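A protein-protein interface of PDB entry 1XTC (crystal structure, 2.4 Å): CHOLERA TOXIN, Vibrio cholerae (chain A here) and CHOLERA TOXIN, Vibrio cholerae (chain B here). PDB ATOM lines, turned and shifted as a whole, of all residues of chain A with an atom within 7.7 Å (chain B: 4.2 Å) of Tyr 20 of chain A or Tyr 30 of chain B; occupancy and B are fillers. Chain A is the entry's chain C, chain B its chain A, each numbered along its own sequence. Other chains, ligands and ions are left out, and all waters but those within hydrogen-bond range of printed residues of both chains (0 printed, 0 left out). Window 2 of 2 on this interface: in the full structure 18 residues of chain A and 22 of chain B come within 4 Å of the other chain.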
ATOM      1  N   VAL A  14     -21.374   9.176   0.571  1.00  0.00           N
ATOM      2  CA  VAL A  14     -21.164   8.581  -0.767  1.00  0.00           C
ATOM      3  C   VAL A  14     -20.915   9.676  -1.815  1.00  0.00           C
ATOM      4  O   VAL A  14     -19.975   9.595  -2.624  1.00  0.00           O
ATOM      5  CB  VAL A  14     -22.356   7.709  -1.134  1.00  0.00           C
ATOM      6  CG1 VAL A  14     -22.426   7.390  -2.625  1.00  0.00           C
ATOM      7  CG2 VAL A  14     -22.319   6.356  -0.412  1.00  0.00           C
ATOM      8  N   LYS A  15     -21.778  10.665  -1.749  1.00  0.00           N
ATOM      9  CA  LYS A  15     -21.734  11.833  -2.622  1.00  0.00           C
ATOM     10  C   LYS A  15     -20.346  12.460  -2.490  1.00  0.00           C
ATOM     11  O   LYS A  15     -19.646  12.695  -3.485  1.00  0.00           O
ATOM     12  CB  LYS A  15     -22.829  12.786  -2.116  1.00  0.00           C
ATOM     13  CG  LYS A  15     -22.952  14.114  -2.853  1.00  0.00           C
ATOM     14  CD  LYS A  15     -23.909  15.083  -2.135  1.00  0.00           C
ATOM     15  CE  LYS A  15     -23.250  16.420  -1.801  1.00  0.00           C
ATOM     16  NZ  LYS A  15     -24.070  17.260  -0.918  1.00  0.00           N
ATOM     17  N   PHE A  16     -19.949  12.677  -1.243  1.00  0.00           N
ATOM     18  CA  PHE A  16     -18.650  13.293  -0.965  1.00  0.00           C
ATOM     19  C   PHE A  16     -17.520  12.449  -1.582  1.00  0.00           C
ATOM     20  O   PHE A  16     -16.678  12.965  -2.320  1.00  0.00           O
ATOM     21  CB  PHE A  16     -18.403  13.426   0.548  1.00  0.00           C
ATOM     22  CG  PHE A  16     -17.012  14.000   0.848  1.00  0.00           C
ATOM     23  CD1 PHE A  16     -16.823  15.386   0.957  1.00  0.00           C
ATOM     24  CD2 PHE A  16     -15.922  13.137   1.004  1.00  0.00           C
ATOM     25  CE1 PHE A  16     -15.540  15.906   1.163  1.00  0.00           C
ATOM     26  CE2 PHE A  16     -14.641  13.657   1.229  1.00  0.00           C
ATOM     27  CZ  PHE A  16     -14.449  15.041   1.297  1.00  0.00           C
ATOM     28  N   LEU A  17     -17.543  11.158  -1.289  1.00  0.00           N
ATOM     29  CA  LEU A  17     -16.518  10.189  -1.768  1.00  0.00           C
ATOM     30  C   LEU A  17     -16.441  10.164  -3.311  1.00  0.00           C
ATOM     31  O   LEU A  17     -15.360  10.042  -3.900  1.00  0.00           O
ATOM     32  CB  LEU A  17     -16.794   8.781  -1.218  1.00  0.00           C
ATOM     33  CG  LEU A  17     -15.700   7.752  -1.570  1.00  0.00           C
ATOM     34  CD1 LEU A  17     -14.272   8.204  -1.238  1.00  0.00           C
ATOM     35  CD2 LEU A  17     -15.882   6.413  -0.841  1.00  0.00           C
ATOM     36  N   ASP A  18     -17.592  10.219  -3.960  1.00  0.00           N
ATOM     37  CA  ASP A  18     -17.670  10.171  -5.439  1.00  0.00           C
ATOM     38  C   ASP A  18     -16.905  11.328  -6.157  1.00  0.00           C
ATOM     39  O   ASP A  18     -16.064  11.073  -7.039  1.00  0.00           O
ATOM     40  CB  ASP A  18     -19.134  10.089  -5.828  1.00  0.00           C
ATOM     41  CG  ASP A  18     -19.668   8.724  -5.419  1.00  0.00           C
ATOM     42  OD1 ASP A  18     -18.826   7.810  -5.053  1.00  0.00           O
ATOM     43  OD2 ASP A  18     -20.923   8.476  -5.432  1.00  0.00           O
ATOM     44  N   GLU A  19     -17.187  12.572  -5.766  1.00  0.00           N
ATOM     45  CA  GLU A  19     -16.532  13.795  -6.341  1.00  0.00           C
ATOM     46  C   GLU A  19     -15.015  13.780  -6.131  1.00  0.00           C
ATOM     47  O   GLU A  19     -14.246  14.205  -6.996  1.00  0.00           O
ATOM     48  CB  GLU A  19     -17.083  15.104  -5.755  1.00  0.00           C
ATOM     49  CG  GLU A  19     -18.089  15.774  -6.704  1.00  0.00           C
ATOM     50  CD  GLU A  19     -19.324  14.914  -6.828  1.00  0.00           C
ATOM     51  OE1 GLU A  19     -19.650  14.173  -5.829  1.00  0.00           O
ATOM     52  OE2 GLU A  19     -20.015  14.912  -7.907  1.00  0.00           O
ATOM     53  N   TYR A  20     -14.593  13.379  -4.948  1.00  0.00           N
ATOM     54  CA  TYR A  20     -13.155  13.241  -4.640  1.00  0.00           C
ATOM     55  C   TYR A  20     -12.489  12.184  -5.565  1.00  0.00           C
ATOM     56  O   TYR A  20     -11.371  12.370  -6.076  1.00  0.00           O
ATOM     57  CB  TYR A  20     -12.927  12.956  -3.168  1.00  0.00           C
ATOM     58  CG  TYR A  20     -11.445  12.993  -2.830  1.00  0.00           C
ATOM     59  CD1 TYR A  20     -10.804  14.200  -2.477  1.00  0.00           C
ATOM     60  CD2 TYR A  20     -10.728  11.811  -2.898  1.00  0.00           C
ATOM     61  CE1 TYR A  20      -9.425  14.194  -2.188  1.00  0.00           C
ATOM     62  CE2 TYR A  20      -9.360  11.802  -2.616  1.00  0.00           C
ATOM     63  CZ  TYR A  20      -8.708  12.989  -2.258  1.00  0.00           C
ATOM     64  OH  TYR A  20      -7.378  12.957  -1.986  1.00  0.00           O
ATOM     65  N   GLN A  21     -13.171  11.063  -5.749  1.00  0.00           N
ATOM     66  CA  GLN A  21     -12.685  10.004  -6.644  1.00  0.00           C
ATOM     67  C   GLN A  21     -12.446  10.655  -8.033  1.00  0.00           C
ATOM     68  O   GLN A  21     -11.419  10.400  -8.681  1.00  0.00           O
ATOM     69  CB  GLN A  21     -13.647   8.808  -6.599  1.00  0.00           C
ATOM     70  CG  GLN A  21     -13.516   8.075  -5.256  1.00  0.00           C
ATOM     71  CD  GLN A  21     -14.169   6.699  -5.206  1.00  0.00           C
ATOM     72  OE1 GLN A  21     -13.585   5.762  -4.659  1.00  0.00           O
ATOM     73  NE2 GLN A  21     -15.364   6.530  -5.730  1.00  0.00           N
ATOM     74  N   SER A  22     -13.406  11.502  -8.476  1.00  0.00           N
ATOM     75  CA  SER A  22     -13.281  12.272  -9.761  1.00  0.00           C
ATOM     76  C   SER A  22     -12.020  13.192  -9.744  1.00  0.00           C
ATOM     77  O   SER A  22     -11.227  13.262 -10.667  1.00  0.00           O
ATOM     78  CB  SER A  22     -14.548  13.071 -10.059  1.00  0.00           C
ATOM     79  OG  SER A  22     -15.590  12.164 -10.423  1.00  0.00           O
ATOM     80  N   LYS A  23     -11.712  13.990  -8.730  1.00  0.00           N
ATOM     81  CA  LYS A  23     -10.390  14.667  -8.853  1.00  0.00           C
ATOM     82  C   LYS A  23      -9.195  13.615  -8.950  1.00  0.00           C
ATOM     83  O   LYS A  23      -8.288  13.739  -9.768  1.00  0.00           O
ATOM     84  CB  LYS A  23     -10.038  15.644  -7.726  1.00  0.00           C
ATOM     85  CG  LYS A  23     -11.212  16.105  -6.885  1.00  0.00           C
ATOM     86  CD  LYS A  23     -11.628  17.561  -7.118  1.00  0.00           C
ATOM     87  CE  LYS A  23     -11.791  18.356  -5.820  1.00  0.00           C
ATOM     88  NZ  LYS A  23     -12.812  17.793  -4.924  1.00  0.00           N
ATOM     89  N   VAL A  24      -9.109  12.525  -8.091  1.00  0.00           N
ATOM     90  CA  VAL A  24      -7.906  11.552  -8.137  1.00  0.00           C
ATOM     91  C   VAL A  24      -7.715  10.908  -9.514  1.00  0.00           C
ATOM     92  O   VAL A  24      -6.618  10.944 -10.105  1.00  0.00           O
ATOM     93  CB  VAL A  24      -8.053  10.328  -7.195  1.00  0.00           C
ATOM     94  CG1 VAL A  24      -6.746   9.527  -7.016  1.00  0.00           C
ATOM     95  CG2 VAL A  24      -8.500  10.700  -5.786  1.00  0.00           C
ATOM     96  N   LYS A  25      -8.809  10.353  -9.987  1.00  0.00           N
ATOM     97  CA  LYS A  25      -8.843   9.691 -11.282  1.00  0.00           C
ATOM     98  C   LYS A  25      -8.417  10.676 -12.349  1.00  0.00           C
ATOM     99  O   LYS A  25      -7.553  10.382 -13.184  1.00  0.00           O
ATOM    100  CB  LYS A  25     -10.256   9.212 -11.601  1.00  0.00           C
ATOM    101  CG  LYS A  25     -10.581   7.836 -11.023  1.00  0.00           C
ATOM    102  CD  LYS A  25     -12.044   7.457 -11.242  1.00  0.00           C
ATOM    103  CE  LYS A  25     -12.221   6.144 -12.002  1.00  0.00           C
ATOM    104  NZ  LYS A  25     -13.634   5.789 -12.195  1.00  0.00           N
ATOM    105  N   ARG A  26      -9.019  11.845 -12.276  1.00  0.00           N
ATOM    106  CA  ARG A  26      -8.767  12.881 -13.268  1.00  0.00           C
ATOM    107  C   ARG A  26      -7.277  13.220 -13.359  1.00  0.00           C
ATOM    108  O   ARG A  26      -6.737  13.350 -14.461  1.00  0.00           O
ATOM    109  CB  ARG A  26      -9.475  14.182 -12.936  1.00  0.00           C
ATOM    110  CG  ARG A  26      -8.889  15.330 -13.755  1.00  0.00           C
ATOM    111  CD  ARG A  26      -9.607  16.629 -13.513  1.00  0.00           C
ATOM    112  NE  ARG A  26      -8.759  17.813 -13.651  1.00  0.00           N
ATOM    113  CZ  ARG A  26      -9.221  18.916 -14.219  1.00  0.00           C
ATOM    114  NH1 ARG A  26     -10.461  18.928 -14.733  1.00  0.00           N
ATOM    115  NH2 ARG A  26      -8.553  20.064 -14.288  1.00  0.00           N
ATOM    116  N   SER B  19      -4.250  -2.795  -4.027  1.00  0.00           N
ATOM    117  CA  SER B  19      -5.482  -2.301  -3.415  1.00  0.00           C
ATOM    118  C   SER B  19      -5.953  -0.962  -3.950  1.00  0.00           C
ATOM    119  O   SER B  19      -7.149  -0.613  -3.817  1.00  0.00           O
ATOM    120  CB  SER B  19      -5.423  -2.323  -1.907  1.00  0.00           C
ATOM    121  OG  SER B  19      -5.611  -3.616  -1.391  1.00  0.00           O
ATOM    122  N   GLY B  20      -4.916   0.035  -4.420  1.00  0.00           N
ATOM    123  CA  GLY B  20      -5.064   1.424  -4.875  1.00  0.00           C
ATOM    124  C   GLY B  20      -4.706   2.372  -3.736  1.00  0.00           C
ATOM    125  O   GLY B  20      -4.840   3.590  -3.867  1.00  0.00           O
ATOM    126  N   MET B  23      -7.104   1.077   2.515  1.00  0.00           N
ATOM    127  CA  MET B  23      -8.554   1.032   2.617  1.00  0.00           C
ATOM    128  C   MET B  23      -9.091   0.779   4.038  1.00  0.00           C
ATOM    129  O   MET B  23      -8.583  -0.025   4.832  1.00  0.00           O
ATOM    130  CB  MET B  23      -9.205   0.016   1.689  1.00  0.00           C
ATOM    131  CG  MET B  23      -8.813  -0.087   0.287  1.00  0.00           C
ATOM    132  SD  MET B  23      -8.926   1.484  -0.599  1.00  0.00           S
ATOM    133  CE  MET B  23      -7.213   2.059  -0.507  1.00  0.00           C
ATOM    134  N   GLU B  29     -10.640  -2.602  -3.587  1.00  0.00           N
ATOM    135  CA  GLU B  29     -10.155  -1.735  -4.678  1.00  0.00           C
ATOM    136  C   GLU B  29     -10.711  -0.336  -4.396  1.00  0.00           C
ATOM    137  O   GLU B  29     -11.893  -0.139  -4.001  1.00  0.00           O
ATOM    138  CB  GLU B  29     -10.606  -2.260  -6.040  1.00  0.00           C
ATOM    139  CG  GLU B  29     -10.834  -3.730  -6.307  1.00  0.00           C
ATOM    140  CD  GLU B  29      -9.931  -4.603  -7.086  1.00  0.00           C
ATOM    141  OE1 GLU B  29      -9.699  -4.247  -8.283  1.00  0.00           O
ATOM    142  OE2 GLU B  29      -9.516  -5.722  -6.732  1.00  0.00           O
ATOM    143  N   TYR B  30      -9.870   0.674  -4.470  1.00  0.00           N
ATOM    144  CA  TYR B  30     -10.203   2.048  -4.191  1.00  0.00           C
ATOM    145  C   TYR B  30     -11.295   2.678  -5.004  1.00  0.00           C
ATOM    146  O   TYR B  30     -11.905   3.701  -4.570  1.00  0.00           O
ATOM    147  CB  TYR B  30      -8.906   2.926  -4.220  1.00  0.00           C
ATOM    148  CG  TYR B  30      -9.208   4.372  -3.877  1.00  0.00           C
ATOM    149  CD1 TYR B  30      -9.659   4.725  -2.597  1.00  0.00           C
ATOM    150  CD2 TYR B  30      -9.182   5.347  -4.871  1.00  0.00           C
ATOM    151  CE1 TYR B  30     -10.153   6.007  -2.338  1.00  0.00           C
ATOM    152  CE2 TYR B  30      -9.623   6.634  -4.610  1.00  0.00           C
ATOM    153  CZ  TYR B  30     -10.092   6.968  -3.337  1.00  0.00           C
ATOM    154  OH  TYR B  30     -10.464   8.265  -3.134  1.00  0.00           O
ATOM    155  N   PHE B  31     -11.649   2.144  -6.158  1.00  0.00           N
ATOM    156  CA  PHE B  31     -12.609   2.782  -7.063  1.00  0.00           C
ATOM    157  C   PHE B  31     -13.964   2.152  -7.173  1.00  0.00           C
ATOM    158  O   PHE B  31     -14.692   2.437  -8.176  1.00  0.00           O
ATOM    159  CB  PHE B  31     -11.976   3.089  -8.409  1.00  0.00           C
ATOM    160  CG  PHE B  31     -10.898   4.115  -8.467  1.00  0.00           C
ATOM    161  CD1 PHE B  31     -11.132   5.431  -8.067  1.00  0.00           C
ATOM    162  CD2 PHE B  31      -9.653   3.796  -9.003  1.00  0.00           C
ATOM    163  CE1 PHE B  31     -10.151   6.409  -8.252  1.00  0.00           C
ATOM    164  CE2 PHE B  31      -8.671   4.748  -9.203  1.00  0.00           C
ATOM    165  CZ  PHE B  31      -8.900   6.047  -8.789  1.00  0.00           C
ATOM    166  N   ASP B  32     -14.440   1.450  -6.167  1.00  0.00           N
ATOM    167  CA  ASP B  32     -15.807   0.871  -6.218  1.00  0.00           C
ATOM    168  C   ASP B  32     -16.878   1.862  -5.764  1.00  0.00           C
ATOM    169  O   ASP B  32     -17.052   1.972  -4.523  1.00  0.00           O
ATOM    170  CB  ASP B  32     -15.856  -0.334  -5.233  1.00  0.00           C
ATOM    171  CG  ASP B  32     -15.106  -1.480  -5.889  1.00  0.00           C
ATOM    172  OD1 ASP B  32     -15.619  -1.964  -6.915  1.00  0.00           O
ATOM    173  OD2 ASP B  32     -13.936  -1.571  -5.481  1.00  0.00           O
ATOM    174  N   ALA B  91      -4.442  15.925   2.059  1.00  0.00           N
ATOM    175  CA  ALA B  91      -5.478  16.269   1.125  1.00  0.00           C
ATOM    176  C   ALA B  91      -6.828  16.469   1.801  1.00  0.00           C
ATOM    177  O   ALA B  91      -7.130  16.098   2.936  1.00  0.00           O
ATOM    178  CB  ALA B  91      -5.514  15.320  -0.069  1.00  0.00           C
ATOM    179  N   ASN B  93      -9.548  15.194   1.737  1.00  0.00           N
ATOM    180  CA  ASN B  93     -10.487  14.099   2.045  1.00  0.00           C
ATOM    181  C   ASN B  93     -10.238  13.595   3.484  1.00  0.00           C
ATOM    182  O   ASN B  93     -10.713  12.506   3.830  1.00  0.00           O
ATOM    183  CB  ASN B  93     -10.439  13.002   1.012  1.00  0.00           C
ATOM    184  CG  ASN B  93      -9.106  12.312   0.967  1.00  0.00           C
ATOM    185  OD1 ASN B  93      -8.078  13.001   1.020  1.00  0.00           O
ATOM    186  ND2 ASN B  93      -9.119  10.988   0.900  1.00  0.00           N
ATOM    187  N   GLY B 117     -13.201   7.251   2.902  1.00  0.00           N
ATOM    188  CA  GLY B 117     -12.986   6.327   1.793  1.00  0.00           C
ATOM    189  C   GLY B 117     -11.636   5.647   1.768  1.00  0.00           C
ATOM    190  O   GLY B 117     -11.519   4.595   1.085  1.00  0.00           O
ATOM    191  N   PRO B 120      -5.713   6.768  -1.331  1.00  0.00           N
ATOM    192  CA  PRO B 120      -5.187   6.382  -2.635  1.00  0.00           C
ATOM    193  C   PRO B 120      -3.653   6.382  -2.653  1.00  0.00           C
ATOM    194  O   PRO B 120      -3.038   7.446  -2.545  1.00  0.00           O
ATOM    195  CB  PRO B 120      -5.675   7.489  -3.576  1.00  0.00           C
ATOM    196  CG  PRO B 120      -6.226   8.574  -2.725  1.00  0.00           C
ATOM    197  CD  PRO B 120      -6.723   7.840  -1.474  1.00  0.00           C
ATOM    198  N   GLN B 123      -1.539   9.333  -2.781  1.00  0.00           N
ATOM    199  CA  GLN B 123      -1.407  10.033  -1.498  1.00  0.00           C
ATOM    200  C   GLN B 123      -0.208   9.524  -0.703  1.00  0.00           C
ATOM    201  O   GLN B 123       0.625  10.326  -0.273  1.00  0.00           O
ATOM    202  CB  GLN B 123      -2.674  10.090  -0.650  1.00  0.00           C
ATOM    203  CG  GLN B 123      -3.184  11.535  -0.512  1.00  0.00           C
ATOM    204  CD  GLN B 123      -4.522  11.642   0.150  1.00  0.00           C
ATOM    205  OE1 GLN B 123      -5.498  10.954  -0.169  1.00  0.00           O
ATOM    206  NE2 GLN B 123      -4.594  12.574   1.124  1.00  0.00           N
ATOM    207  N   TYR B 150       0.132  17.335  -4.560  1.00  0.00           N
ATOM    208  CA  TYR B 150      -0.013  17.196  -3.117  1.00  0.00           C
ATOM    209  C   TYR B 150       0.612  18.287  -2.287  1.00  0.00           C
ATOM    210  O   TYR B 150      -0.100  18.820  -1.378  1.00  0.00           O
ATOM    211  CB  TYR B 150       0.126  15.776  -2.592  1.00  0.00           C
ATOM    212  CG  TYR B 150      -1.001  14.844  -2.988  1.00  0.00           C
ATOM    213  CD1 TYR B 150      -2.338  15.144  -2.706  1.00  0.00           C
ATOM    214  CD2 TYR B 150      -0.725  13.627  -3.627  1.00  0.00           C
ATOM    215  CE1 TYR B 150      -3.378  14.313  -3.162  1.00  0.00           C
ATOM    216  CE2 TYR B 150      -1.736  12.781  -4.078  1.00  0.00           C
ATOM    217  CZ  TYR B 150      -3.054  13.130  -3.846  1.00  0.00           C
ATOM    218  OH  TYR B 150      -4.032  12.249  -4.232  1.00  0.00           O
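O of Ser 19 of chain B sits at hydrogen-bond distance from N of Tyr 30 of chain B (3.1 Å).
N of Ala 91 of chain B sits close to NE2 of Gln 123 of chain B, at 3.5 Å.
Hydrophobic or aromatic side chains of chain B within 4 Å of the printed part of chain A: Tyr 30, Phe 31 and Ala 91.
Along chain B the printed residues that touch a printed residue of chain A span positions 30 to 123.
Hydrophobic or aromatic side chains of chain A that line the printed part of chain B: Leu 17 and Tyr 20.
Gly 117 of chain B touches Leu 17 of chain A (CA to CD1, 3.8 Å).
Tyr 30 of chain B touches Tyr 20 of chain A.
OH of Tyr 20 of chain A touches CB of Ala 91 of chain B, 3.6 Å away.
OE1 of Gln 21 of chain A touches CA of Phe 31 of chain B, at 3.95 Å.
Lys 25 of chain A touches Phe 31 of chain B (CG to CE1, 3.1 Å).
Of chain B, only Tyr 30 (3.6 Å), Ala 91 (3.6 Å), Asn 93 (3.1 Å) and Gln 123 (3.3 Å) come within 4 Å of Tyr 20 of chain A.
Printed residues of chain B within 4 Å of Gln 21 of chain A: Tyr 30 and Phe 31.
Printed residues of chain A within 4 Å of Tyr 30 of chain B: Tyr 20 and Gln 21.
Printed residues of chain A within 4 Å of Ala 91 of chain B: Tyr 20.
Of the printed residues of chain A, Asn 93 of chain B touches Tyr 20 (3.1 Å).
Of the printed residues of chain A, Gly 117 of chain B touches Leu 17.
Of the printed residues of chain A, Gln 123 of chain B touches Tyr 20.
The side-chain amide oxygen (OE1) of Gln 21 of chain A sits close to the backbone carbonyl oxygen (O) of Tyr 30 of chain B, 2.7 Å away.
OH of Tyr 20 of chain A is in hydrogen-bond range of OD1 of Asn 93 of chain B (3.1 Å).
The side-chain amide oxygen (OE1) of Gln 123 of chain B is in hydrogen-bond range of the side-chain hydroxyl (OH) of Tyr 20 of chain A, 3.3 Å away.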
